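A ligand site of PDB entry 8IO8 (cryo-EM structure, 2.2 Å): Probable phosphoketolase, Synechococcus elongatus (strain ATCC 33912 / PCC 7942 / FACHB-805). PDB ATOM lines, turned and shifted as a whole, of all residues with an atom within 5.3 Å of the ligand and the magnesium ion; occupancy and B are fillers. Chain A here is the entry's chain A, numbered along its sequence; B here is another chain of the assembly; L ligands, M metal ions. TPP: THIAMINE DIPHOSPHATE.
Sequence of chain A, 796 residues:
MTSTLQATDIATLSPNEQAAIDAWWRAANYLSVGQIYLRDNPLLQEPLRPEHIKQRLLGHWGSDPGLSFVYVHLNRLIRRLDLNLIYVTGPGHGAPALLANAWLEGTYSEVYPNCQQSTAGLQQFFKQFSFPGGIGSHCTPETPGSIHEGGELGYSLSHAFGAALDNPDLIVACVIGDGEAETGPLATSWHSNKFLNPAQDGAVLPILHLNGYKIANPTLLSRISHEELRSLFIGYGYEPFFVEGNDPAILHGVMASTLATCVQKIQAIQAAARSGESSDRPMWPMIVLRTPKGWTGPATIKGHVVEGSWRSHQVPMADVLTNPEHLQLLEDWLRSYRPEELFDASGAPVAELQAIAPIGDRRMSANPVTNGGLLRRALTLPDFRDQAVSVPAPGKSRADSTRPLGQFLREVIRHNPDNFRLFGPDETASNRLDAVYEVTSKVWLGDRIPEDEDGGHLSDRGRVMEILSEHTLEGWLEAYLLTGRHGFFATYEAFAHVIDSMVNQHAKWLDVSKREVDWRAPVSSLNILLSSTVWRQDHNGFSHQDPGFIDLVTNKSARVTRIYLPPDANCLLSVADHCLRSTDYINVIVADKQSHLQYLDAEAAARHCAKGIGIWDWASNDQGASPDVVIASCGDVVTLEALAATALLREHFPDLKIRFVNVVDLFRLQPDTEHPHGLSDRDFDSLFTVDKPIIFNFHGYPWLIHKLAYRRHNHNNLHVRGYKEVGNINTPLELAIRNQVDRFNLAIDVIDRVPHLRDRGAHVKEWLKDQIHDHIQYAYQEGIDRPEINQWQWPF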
ATOM      1  N   GLY A  62      21.966 -19.670  20.621  1.00  0.00           N
ATOM      2  CA  GLY A  62      22.074 -20.528  19.443  1.00  0.00           C
ATOM      3  C   GLY A  62      22.971 -19.962  18.363  1.00  0.00           C
ATOM      4  O   GLY A  62      23.740 -20.692  17.743  1.00  0.00           O
ATOM      5  N   SER A  63      22.897 -18.655  18.132  1.00  0.00           N
ATOM      6  CA  SER A  63      23.677 -18.050  17.059  1.00  0.00           C
ATOM      7  C   SER A  63      25.092 -17.680  17.468  1.00  0.00           C
ATOM      8  O   SER A  63      25.920 -17.428  16.594  1.00  0.00           O
ATOM      9  CB  SER A  63      22.950 -16.814  16.531  1.00  0.00           C
ATOM     10  OG  SER A  63      23.461 -16.418  15.279  1.00  0.00           O
ATOM     11  N   PRO A  91      22.060 -11.618  12.833  1.00  0.00           N
ATOM     12  CA  PRO A  91      21.416 -12.053  14.072  1.00  0.00           C
ATOM     13  C   PRO A  91      21.831 -11.198  15.251  1.00  0.00           C
ATOM     14  O   PRO A  91      22.741 -11.556  15.995  1.00  0.00           O
ATOM     15  CB  PRO A  91      21.904 -13.505  14.239  1.00  0.00           C
ATOM     16  CG  PRO A  91      22.423 -13.899  12.906  1.00  0.00           C
ATOM     17  CD  PRO A  91      22.968 -12.649  12.309  1.00  0.00           C
ATOM     18  N   HIS A  93      20.527 -10.746  18.018  1.00  0.00           N
ATOM     19  CA  HIS A  93      20.412 -11.433  19.288  1.00  0.00           C
ATOM     20  C   HIS A  93      21.693 -12.166  19.675  1.00  0.00           C
ATOM     21  O   HIS A  93      21.829 -12.594  20.824  1.00  0.00           O
ATOM     22  CB  HIS A  93      19.234 -12.402  19.259  1.00  0.00           C
ATOM     23  CG  HIS A  93      19.264 -13.338  18.093  1.00  0.00           C
ATOM     24  ND1 HIS A  93      18.837 -12.980  16.838  1.00  0.00           N
ATOM     25  CD2 HIS A  93      19.651 -14.632  17.994  1.00  0.00           C
ATOM     26  CE1 HIS A  93      18.961 -13.993  16.014  1.00  0.00           C
ATOM     27  NE2 HIS A  93      19.455 -15.019  16.691  1.00  0.00           N
ATOM     28  N   GLY A 150      20.460  -6.142  15.024  1.00  0.00           N
ATOM     29  CA  GLY A 150      19.613  -7.102  14.347  1.00  0.00           C
ATOM     30  C   GLY A 150      18.328  -7.373  15.098  1.00  0.00           C
ATOM     31  O   GLY A 150      17.875  -8.518  15.144  1.00  0.00           O
ATOM     32  N   GLY A 151      17.748  -6.340  15.697  1.00  0.00           N
ATOM     33  CA  GLY A 151      16.478  -6.488  16.373  1.00  0.00           C
ATOM     34  C   GLY A 151      15.368  -6.758  15.383  1.00  0.00           C
ATOM     35  O   GLY A 151      14.692  -7.791  15.449  1.00  0.00           O
ATOM     36  N   GLU A 152      15.172  -5.822  14.456  1.00  0.00           N
ATOM     37  CA  GLU A 152      14.268  -6.015  13.333  1.00  0.00           C
ATOM     38  C   GLU A 152      15.060  -6.612  12.179  1.00  0.00           C
ATOM     39  O   GLU A 152      15.972  -5.969  11.644  1.00  0.00           O
ATOM     40  CB  GLU A 152      13.622  -4.684  12.934  1.00  0.00           C
ATOM     41  CG  GLU A 152      12.645  -4.799  11.791  1.00  0.00           C
ATOM     42  CD  GLU A 152      11.366  -5.472  12.193  1.00  0.00           C
ATOM     43  OE1 GLU A 152      10.794  -5.088  13.232  1.00  0.00           O
ATOM     44  OE2 GLU A 152      10.927  -6.397  11.482  1.00  0.00           O
ATOM     45  N   LEU A 153      14.735  -7.837  11.810  1.00  0.00           N
ATOM     46  CA  LEU A 153      15.543  -8.580  10.853  1.00  0.00           C
ATOM     47  C   LEU A 153      15.211  -8.178   9.418  1.00  0.00           C
ATOM     48  O   LEU A 153      14.103  -7.713   9.120  1.00  0.00           O
ATOM     49  CB  LEU A 153      15.332 -10.076  11.045  1.00  0.00           C
ATOM     50  CG  LEU A 153      15.769 -10.602  12.405  1.00  0.00           C
ATOM     51  CD1 LEU A 153      15.344 -12.045  12.562  1.00  0.00           C
ATOM     52  CD2 LEU A 153      17.267 -10.466  12.593  1.00  0.00           C
ATOM     53  N   GLY A 177      21.616 -14.503   9.230  1.00  0.00           N
ATOM     54  CA  GLY A 177      20.923 -15.664   9.738  1.00  0.00           C
ATOM     55  C   GLY A 177      19.960 -16.233   8.710  1.00  0.00           C
ATOM     56  O   GLY A 177      19.335 -15.503   7.942  1.00  0.00           O
ATOM     57  N   ASP A 178      19.857 -17.559   8.690  1.00  0.00           N
ATOM     58  CA  ASP A 178      19.007 -18.201   7.691  1.00  0.00           C
ATOM     59  C   ASP A 178      17.532 -17.895   7.923  1.00  0.00           C
ATOM     60  O   ASP A 178      16.745 -17.880   6.970  1.00  0.00           O
ATOM     61  CB  ASP A 178      19.251 -19.707   7.676  1.00  0.00           C
ATOM     62  CG  ASP A 178      19.277 -20.310   9.057  1.00  0.00           C
ATOM     63  OD1 ASP A 178      19.582 -19.594  10.022  1.00  0.00           O
ATOM     64  OD2 ASP A 178      19.004 -21.526   9.173  1.00  0.00           O
ATOM     65  N   GLY A 179      17.125 -17.662   9.174  1.00  0.00           N
ATOM     66  CA  GLY A 179      15.786 -17.169   9.408  1.00  0.00           C
ATOM     67  C   GLY A 179      15.586 -15.767   8.876  1.00  0.00           C
ATOM     68  O   GLY A 179      14.553 -15.465   8.269  1.00  0.00           O
ATOM     69  N   GLU A 180      16.575 -14.897   9.061  1.00  0.00           N
ATOM     70  CA  GLU A 180      16.502 -13.534   8.552  1.00  0.00           C
ATOM     71  C   GLU A 180      16.414 -13.518   7.023  1.00  0.00           C
ATOM     72  O   GLU A 180      15.791 -12.627   6.448  1.00  0.00           O
ATOM     73  CB  GLU A 180      17.709 -12.732   9.020  1.00  0.00           C
ATOM     74  CG  GLU A 180      17.729 -11.291   8.571  1.00  0.00           C
ATOM     75  CD  GLU A 180      19.048 -10.611   8.844  1.00  0.00           C
ATOM     76  OE1 GLU A 180      20.022 -11.318   9.199  1.00  0.00           O
ATOM     77  OE2 GLU A 180      19.123  -9.364   8.716  1.00  0.00           O
ATOM     78  N   THR A 183      13.039 -13.101   5.215  1.00  0.00           N
ATOM     79  CA  THR A 183      12.289 -11.863   5.238  1.00  0.00           C
ATOM     80  C   THR A 183      12.288 -11.205   3.856  1.00  0.00           C
ATOM     81  O   THR A 183      13.141 -11.473   3.007  1.00  0.00           O
ATOM     82  CB  THR A 183      12.854 -10.890   6.274  1.00  0.00           C
ATOM     83  OG1 THR A 183      14.184 -10.527   5.906  1.00  0.00           O
ATOM     84  CG2 THR A 183      12.877 -11.537   7.642  1.00  0.00           C
ATOM     85  N   HIS A 209      24.676 -17.684   7.637  1.00  0.00           N
ATOM     86  CA  HIS A 209      24.783 -18.535   8.812  1.00  0.00           C
ATOM     87  C   HIS A 209      23.624 -19.520   8.784  1.00  0.00           C
ATOM     88  O   HIS A 209      22.565 -19.277   9.361  1.00  0.00           O
ATOM     89  CB  HIS A 209      24.798 -17.713  10.083  1.00  0.00           C
ATOM     90  CG  HIS A 209      25.026 -18.523  11.327  1.00  0.00           C
ATOM     91  ND1 HIS A 209      24.708 -18.063  12.583  1.00  0.00           N
ATOM     92  CD2 HIS A 209      25.533 -19.763  11.488  1.00  0.00           C
ATOM     93  CE1 HIS A 209      25.028 -18.990  13.468  1.00  0.00           C
ATOM     94  NE2 HIS A 209      25.519 -20.038  12.828  1.00  0.00           N
ATOM     95  N   ASN A 211      22.388 -22.315  10.136  1.00  0.00           N
ATOM     96  CA  ASN A 211      22.360 -23.269  11.235  1.00  0.00           C
ATOM     97  C   ASN A 211      21.109 -24.154  11.221  1.00  0.00           C
ATOM     98  O   ASN A 211      20.992 -25.029  12.078  1.00  0.00           O
ATOM     99  CB  ASN A 211      22.490 -22.569  12.588  1.00  0.00           C
ATOM    100  CG  ASN A 211      21.524 -21.415  12.750  1.00  0.00           C
ATOM    101  OD1 ASN A 211      20.528 -21.326  12.046  1.00  0.00           O
ATOM    102  ND2 ASN A 211      21.815 -20.534  13.688  1.00  0.00           N
ATOM    103  N   GLY A 212      20.189 -23.921  10.289  1.00  0.00           N
ATOM    104  CA  GLY A 212      19.080 -24.825  10.056  1.00  0.00           C
ATOM    105  C   GLY A 212      17.793 -24.451  10.750  1.00  0.00           C
ATOM    106  O   GLY A 212      16.758 -25.030  10.419  1.00  0.00           O
ATOM    107  N   TYR A 213      17.817 -23.519  11.685  1.00  0.00           N
ATOM    108  CA  TYR A 213      16.633 -23.188  12.464  1.00  0.00           C
ATOM    109  C   TYR A 213      16.634 -21.689  12.756  1.00  0.00           C
ATOM    110  O   TYR A 213      17.670 -21.029  12.680  1.00  0.00           O
ATOM    111  CB  TYR A 213      16.566 -23.992  13.769  1.00  0.00           C
ATOM    112  CG  TYR A 213      16.540 -25.479  13.567  1.00  0.00           C
ATOM    113  CD1 TYR A 213      15.336 -26.152  13.399  1.00  0.00           C
ATOM    114  CD2 TYR A 213      17.715 -26.222  13.531  1.00  0.00           C
ATOM    115  CE1 TYR A 213      15.310 -27.518  13.215  1.00  0.00           C
ATOM    116  CE2 TYR A 213      17.689 -27.588  13.347  1.00  0.00           C
ATOM    117  CZ  TYR A 213      16.478 -28.225  13.184  1.00  0.00           C
ATOM    118  OH  TYR A 213      16.452 -29.584  13.007  1.00  0.00           O
ATOM    119  N   LYS A 214      15.453 -21.165  13.082  1.00  0.00           N
ATOM    120  CA  LYS A 214      15.338 -19.767  13.470  1.00  0.00           C
ATOM    121  C   LYS A 214      14.905 -19.583  14.920  1.00  0.00           C
ATOM    122  O   LYS A 214      15.687 -19.054  15.720  1.00  0.00           O
ATOM    123  CB  LYS A 214      14.349 -19.067  12.526  1.00  0.00           C
ATOM    124  CG  LYS A 214      13.333 -19.989  11.888  1.00  0.00           C
ATOM    125  CD  LYS A 214      12.419 -19.239  10.933  1.00  0.00           C
ATOM    126  CE  LYS A 214      11.422 -20.178  10.283  1.00  0.00           C
ATOM    127  NZ  LYS A 214      10.567 -19.469   9.297  1.00  0.00           N
ATOM    128  N   ILE A 215      13.709 -20.014  15.298  1.00  0.00           N
ATOM    129  CA  ILE A 215      13.297 -19.983  16.691  1.00  0.00           C
ATOM    130  C   ILE A 215      12.753 -21.344  17.100  1.00  0.00           C
ATOM    131  O   ILE A 215      13.225 -21.956  18.068  1.00  0.00           O
ATOM    132  CB  ILE A 215      12.249 -18.882  16.957  1.00  0.00           C
ATOM    133  CG1 ILE A 215      12.913 -17.507  16.922  1.00  0.00           C
ATOM    134  CG2 ILE A 215      11.577 -19.099  18.300  1.00  0.00           C
ATOM    135  CD1 ILE A 215      12.066 -16.408  17.532  1.00  0.00           C
ATOM    136  N   THR A 219      14.527 -23.454   8.965  1.00  0.00           N
ATOM    137  CA  THR A 219      14.507 -22.400   7.966  1.00  0.00           C
ATOM    138  C   THR A 219      14.367 -23.008   6.574  1.00  0.00           C
ATOM    139  O   THR A 219      14.893 -24.091   6.306  1.00  0.00           O
ATOM    140  CB  THR A 219      15.782 -21.558   8.040  1.00  0.00           C
ATOM    141  OG1 THR A 219      16.925 -22.401   7.892  1.00  0.00           O
ATOM    142  CG2 THR A 219      15.851 -20.867   9.389  1.00  0.00           C
ATOM    143  N   LYS A 293      23.212 -25.447  15.365  1.00  0.00           N
ATOM    144  CA  LYS A 293      22.784 -24.343  16.205  1.00  0.00           C
ATOM    145  C   LYS A 293      23.018 -24.700  17.668  1.00  0.00           C
ATOM    146  O   LYS A 293      22.704 -25.818  18.105  1.00  0.00           O
ATOM    147  CB  LYS A 293      21.319 -24.015  15.962  1.00  0.00           C
ATOM    148  CG  LYS A 293      20.855 -22.742  16.638  1.00  0.00           C
ATOM    149  CD  LYS A 293      19.506 -22.297  16.121  1.00  0.00           C
ATOM    150  CE  LYS A 293      19.128 -20.935  16.672  1.00  0.00           C
ATOM    151  NZ  LYS A 293      17.881 -20.416  16.074  1.00  0.00           N
ATOM    152  N   HIS A 313      18.046 -21.922  20.724  1.00  0.00           N
ATOM    153  CA  HIS A 313      17.983 -20.553  20.209  1.00  0.00           C
ATOM    154  C   HIS A 313      18.125 -19.527  21.332  1.00  0.00           C
ATOM    155  O   HIS A 313      18.971 -18.630  21.259  1.00  0.00           O
ATOM    156  CB  HIS A 313      16.680 -20.339  19.454  1.00  0.00           C
ATOM    157  CG  HIS A 313      16.411 -18.904  19.123  1.00  0.00           C
ATOM    158  ND1 HIS A 313      17.042 -18.256  18.082  1.00  0.00           N
ATOM    159  CD2 HIS A 313      15.590 -17.993  19.698  1.00  0.00           C
ATOM    160  CE1 HIS A 313      16.610 -16.999  18.031  1.00  0.00           C
ATOM    161  NE2 HIS A 313      15.733 -16.824  18.996  1.00  0.00           N
ATOM    162  N   PRO B 425       4.362 -15.794  12.402  1.00  0.00           N
ATOM    163  CA  PRO B 425       5.770 -15.745  11.970  1.00  0.00           C
ATOM    164  C   PRO B 425       6.729 -16.427  12.940  1.00  0.00           C
ATOM    165  O   PRO B 425       7.536 -15.798  13.632  1.00  0.00           O
ATOM    166  CB  PRO B 425       6.027 -14.236  11.866  1.00  0.00           C
ATOM    167  CG  PRO B 425       5.020 -13.597  12.808  1.00  0.00           C
ATOM    168  CD  PRO B 425       4.020 -14.634  13.238  1.00  0.00           C
ATOM    169  N   ASP B 426       6.631 -17.759  12.999  1.00  0.00           N
ATOM    170  CA  ASP B 426       7.453 -18.574  13.880  1.00  0.00           C
ATOM    171  C   ASP B 426       7.335 -18.120  15.326  1.00  0.00           C
ATOM    172  O   ASP B 426       8.309 -18.078  16.081  1.00  0.00           O
ATOM    173  CB  ASP B 426       8.918 -18.573  13.425  1.00  0.00           C
ATOM    174  CG  ASP B 426       9.729 -19.677  14.074  1.00  0.00           C
ATOM    175  OD1 ASP B 426       9.133 -20.574  14.693  1.00  0.00           O
ATOM    176  OD2 ASP B 426      10.976 -19.626  13.981  1.00  0.00           O
ATOM    177  N   GLU B 427       6.105 -17.767  15.719  1.00  0.00           N
ATOM    178  CA  GLU B 427       5.843 -17.302  17.070  1.00  0.00           C
ATOM    179  C   GLU B 427       4.685 -18.028  17.729  1.00  0.00           C
ATOM    180  O   GLU B 427       4.299 -17.651  18.843  1.00  0.00           O
ATOM    181  CB  GLU B 427       5.580 -15.788  17.077  1.00  0.00           C
ATOM    182  CG  GLU B 427       6.800 -14.961  16.702  1.00  0.00           C
ATOM    183  CD  GLU B 427       6.467 -13.496  16.487  1.00  0.00           C
ATOM    184  OE1 GLU B 427       5.269 -13.149  16.507  1.00  0.00           O
ATOM    185  OE2 GLU B 427       7.402 -12.695  16.295  1.00  0.00           O
ATOM    186  N   LEU B 468       8.845 -16.690   8.301  1.00  0.00           N
ATOM    187  CA  LEU B 468       9.333 -15.527   9.035  1.00  0.00           C
ATOM    188  C   LEU B 468       9.015 -14.211   8.351  1.00  0.00           C
ATOM    189  O   LEU B 468       9.273 -13.152   8.927  1.00  0.00           O
ATOM    190  CB  LEU B 468      10.840 -15.632   9.245  1.00  0.00           C
ATOM    191  CG  LEU B 468      11.259 -15.070  10.605  1.00  0.00           C
ATOM    192  CD1 LEU B 468      10.433 -15.743  11.677  1.00  0.00           C
ATOM    193  CD2 LEU B 468      12.736 -15.257  10.858  1.00  0.00           C
ATOM    194  N   GLU B 470       6.640 -11.419   7.523  1.00  0.00           N
ATOM    195  CA  GLU B 470       5.331 -10.862   7.848  1.00  0.00           C
ATOM    196  C   GLU B 470       4.580 -10.411   6.607  1.00  0.00           C
ATOM    197  O   GLU B 470       3.349 -10.489   6.567  1.00  0.00           O
ATOM    198  CB  GLU B 470       5.484  -9.692   8.818  1.00  0.00           C
ATOM    199  CG  GLU B 470       5.716 -10.085  10.261  1.00  0.00           C
ATOM    200  CD  GLU B 470       7.128 -10.549  10.520  1.00  0.00           C
ATOM    201  OE1 GLU B 470       7.978 -10.421   9.615  1.00  0.00           O
ATOM    202  OE2 GLU B 470       7.401 -11.040  11.643  1.00  0.00           O
ATOM    203  N   PHE B 495       6.722  -6.248  15.914  1.00  0.00           N
ATOM    204  CA  PHE B 495       6.895  -6.409  14.476  1.00  0.00           C
ATOM    205  C   PHE B 495       5.621  -6.106  13.699  1.00  0.00           C
ATOM    206  O   PHE B 495       5.467  -6.577  12.571  1.00  0.00           O
ATOM    207  CB  PHE B 495       7.397  -7.811  14.167  1.00  0.00           C
ATOM    208  CG  PHE B 495       8.533  -8.241  15.054  1.00  0.00           C
ATOM    209  CD1 PHE B 495       9.758  -7.620  14.969  1.00  0.00           C
ATOM    210  CD2 PHE B 495       8.350  -9.244  15.990  1.00  0.00           C
ATOM    211  CE1 PHE B 495      10.802  -8.001  15.793  1.00  0.00           C
ATOM    212  CE2 PHE B 495       9.393  -9.632  16.821  1.00  0.00           C
ATOM    213  CZ  PHE B 495      10.610  -9.003  16.714  1.00  0.00           C
ATOM    214  N   VAL B 498       5.792  -3.718  10.421  1.00  0.00           N
ATOM    215  CA  VAL B 498       6.210  -4.293   9.153  1.00  0.00           C
ATOM    216  C   VAL B 498       5.036  -4.359   8.181  1.00  0.00           C
ATOM    217  O   VAL B 498       5.215  -4.173   6.973  1.00  0.00           O
ATOM    218  CB  VAL B 498       6.820  -5.682   9.396  1.00  0.00           C
ATOM    219  CG1 VAL B 498       7.299  -6.292   8.089  1.00  0.00           C
ATOM    220  CG2 VAL B 498       7.967  -5.578  10.372  1.00  0.00           C
ATOM    221  N   ASN B 540      12.765 -12.173  23.005  1.00  0.00           N
ATOM    222  CA  ASN B 540      12.738 -11.704  21.621  1.00  0.00           C
ATOM    223  C   ASN B 540      12.088 -10.329  21.525  1.00  0.00           C
ATOM    224  O   ASN B 540      11.224  -9.983  22.336  1.00  0.00           O
ATOM    225  CB  ASN B 540      11.981 -12.699  20.745  1.00  0.00           C
ATOM    226  CG  ASN B 540      10.478 -12.626  20.919  1.00  0.00           C
ATOM    227  OD1 ASN B 540       9.937 -13.062  21.937  1.00  0.00           O
ATOM    228  ND2 ASN B 540       9.802 -12.061  19.934  1.00  0.00           N
ATOM    229  N   GLY B 541      12.506  -9.548  20.539  1.00  0.00           N
ATOM    230  CA  GLY B 541      11.957  -8.227  20.352  1.00  0.00           C
ATOM    231  C   GLY B 541      12.973  -7.156  20.701  1.00  0.00           C
ATOM    232  O   GLY B 541      13.686  -7.283  21.703  1.00  0.00           O
HETATM  233  N1' TPP L   1      10.179 -11.143  12.627  1.00  0.00           N
HETATM  234  C2' TPP L   1      11.048 -10.200  12.228  1.00  0.00           C
HETATM  235  CM2 TPP L   1      10.763  -9.508  10.935  1.00  0.00           C
HETATM  236  N3' TPP L   1      12.146  -9.831  12.882  1.00  0.00           N
HETATM  237  C4' TPP L   1      12.405 -10.447  14.050  1.00  0.00           C
HETATM  238  N4' TPP L   1      13.516 -10.058  14.696  1.00  0.00           N
HETATM  239  C5' TPP L   1      11.543 -11.458  14.565  1.00  0.00           C
HETATM  240  C6' TPP L   1      10.450 -11.746  13.782  1.00  0.00           C
HETATM  241  C7' TPP L   1      11.796 -12.177  15.857  1.00  0.00           C
HETATM  242  N3  TPP L   1      13.134 -12.825  15.919  1.00  0.00           N
HETATM  243  C2  TPP L   1      14.140 -12.340  16.613  1.00  0.00           C
HETATM  244  S1  TPP L   1      15.513 -13.302  16.481  1.00  0.00           S
HETATM  245  C5  TPP L   1      14.685 -14.408  15.449  1.00  0.00           C
HETATM  246  C4  TPP L   1      13.415 -14.011  15.243  1.00  0.00           C
HETATM  247  CM4 TPP L   1      12.380 -14.681  14.426  1.00  0.00           C
HETATM  248  C6  TPP L   1      15.378 -15.627  14.898  1.00  0.00           C
HETATM  249  C7  TPP L   1      15.780 -15.467  13.449  1.00  0.00           C
HETATM  250  O7  TPP L   1      16.465 -16.675  13.031  1.00  0.00           O
HETATM  251  PA  TPP L   1      17.882 -16.697  12.354  1.00  0.00           P
HETATM  252  O1A TPP L   1      18.030 -18.035  11.655  1.00  0.00           O
HETATM  253  O2A TPP L   1      18.065 -15.500  11.518  1.00  0.00           O
HETATM  254  O3A TPP L   1      18.863 -16.707  13.587  1.00  0.00           O
HETATM  255  PB  TPP L   1      19.904 -17.666  14.294  1.00  0.00           P
HETATM  256  O1B TPP L   1      19.719 -17.382  15.777  1.00  0.00           O
HETATM  257  O2B TPP L   1      19.399 -19.072  13.992  1.00  0.00           O
HETATM  258  O3B TPP L   1      21.292 -17.418  13.799  1.00  0.00           O
HETATM  259 MG    MG M   1      19.159 -19.729  12.029  1.00  0.00          MG
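O1B of the ligand is in hydrogen-bond range of NE2 of His 93 (2.5 Å).
O of Gly 151 is in hydrogen-bond range of N4' of the ligand (2.7 Å).
O2A of the ligand sits at hydrogen-bond distance from N of Gly 179 (3.3 Å).
The side-chain hydroxyl (OG) of Ser 63 lies within hydrogen-bond range of an oxygen (O3B) of the ligand (2.8 Å).
The side-chain amino group (NZ) of Lys 293 is in salt-bridge range of an oxygen (O1B) of the ligand (3.6 Å).
N of Glu 180 lies within hydrogen-bond range of O2A of the ligand, at 2.9 Å.
N3' of the ligand is in hydrogen-bond range of N of Leu 153, 3.4 Å away.
The side-chain carboxylate (OD2) of Asp 178 lies within hydrogen-bond range of the side-chain hydroxyl (OG1) of Thr 219 (2.6 Å).
OD2 of Asp 178 is in hydrogen-bond range of N of Gly 212 (2.9 Å).
A ring nitrogen (ND1) of His 209 lies within hydrogen-bond range of the side-chain hydroxyl (OG) of Ser 63, at 3.4 Å.
NZ of Lys 293 sits at hydrogen-bond distance from O of Lys 214.
The side-chain amino group (NZ) of Lys 293 lies within hydrogen-bond range of a ring nitrogen (ND1) of His 313, at 3.1 Å.
The side-chain hydroxyl (OG1) of Thr 183 lies within hydrogen-bond range of the backbone carbonyl oxygen (O) of Glu 180.
The backbone NH of Ile 215 is in hydrogen-bond range of the side-chain carboxylate of Asp 426 of chain B (3.1 Å).
The backbone carbonyl oxygen (O) of His 313 sits at hydrogen-bond distance from the backbone NH (N) of Gly 62 (3.2 Å).
OE2 of Glu 470 of chain B sits close to N1' of the ligand (2.9 Å).
Merely in contact with the ligand: Pro 91 (3.8 Å), Glu 152 (3.2 Å), Gly 177 (3.4 Å), His 209 (3.7 Å), Lys 214 (3.2 Å), Ile 215 (3.6 Å), His 313 (3.6 Å), Leu 468 of chain B (3.5 Å) and Phe 495 of chain B (3.4 Å).
Within 4 Å of the ligand: Ser 63, Pro 91, His 93, Gly 151, Glu 152, Leu 153, Gly 177, Asp 178, Gly 179, Glu 180, His 209, Asn 211, Tyr 213, Lys 214, Ile 215, Lys 293, His 313, Leu 468 of chain B, Glu 470 of chain B and Phe 495 of chain B.
Along chain A the residues within 4 Å of the ligand span positions 63 to 313.
The nearest printed residue that does not touch the ligand is Glu 427 of chain B (4.1 Å).
Of the 31 residues printed, 3 come within 4 Å of the magnesium ion.
The nearest printed residue that does not touch the magnesium ion is Gly 179 (4.1 Å).
The magnesium ion is bound by OD1 of Asp 178, 2.1 Å away.
The magnesium ion is bound by an oxygen (O1A) of the ligand.
The backbone carbonyl oxygen (O) of Tyr 213 binds the magnesium ion, 2.1 Å away.
An oxygen (O2B) of the ligand is bound to the magnesium ion (2.1 Å).
The magnesium ion is bound by OD1 of Asn 211 (2.1 Å).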
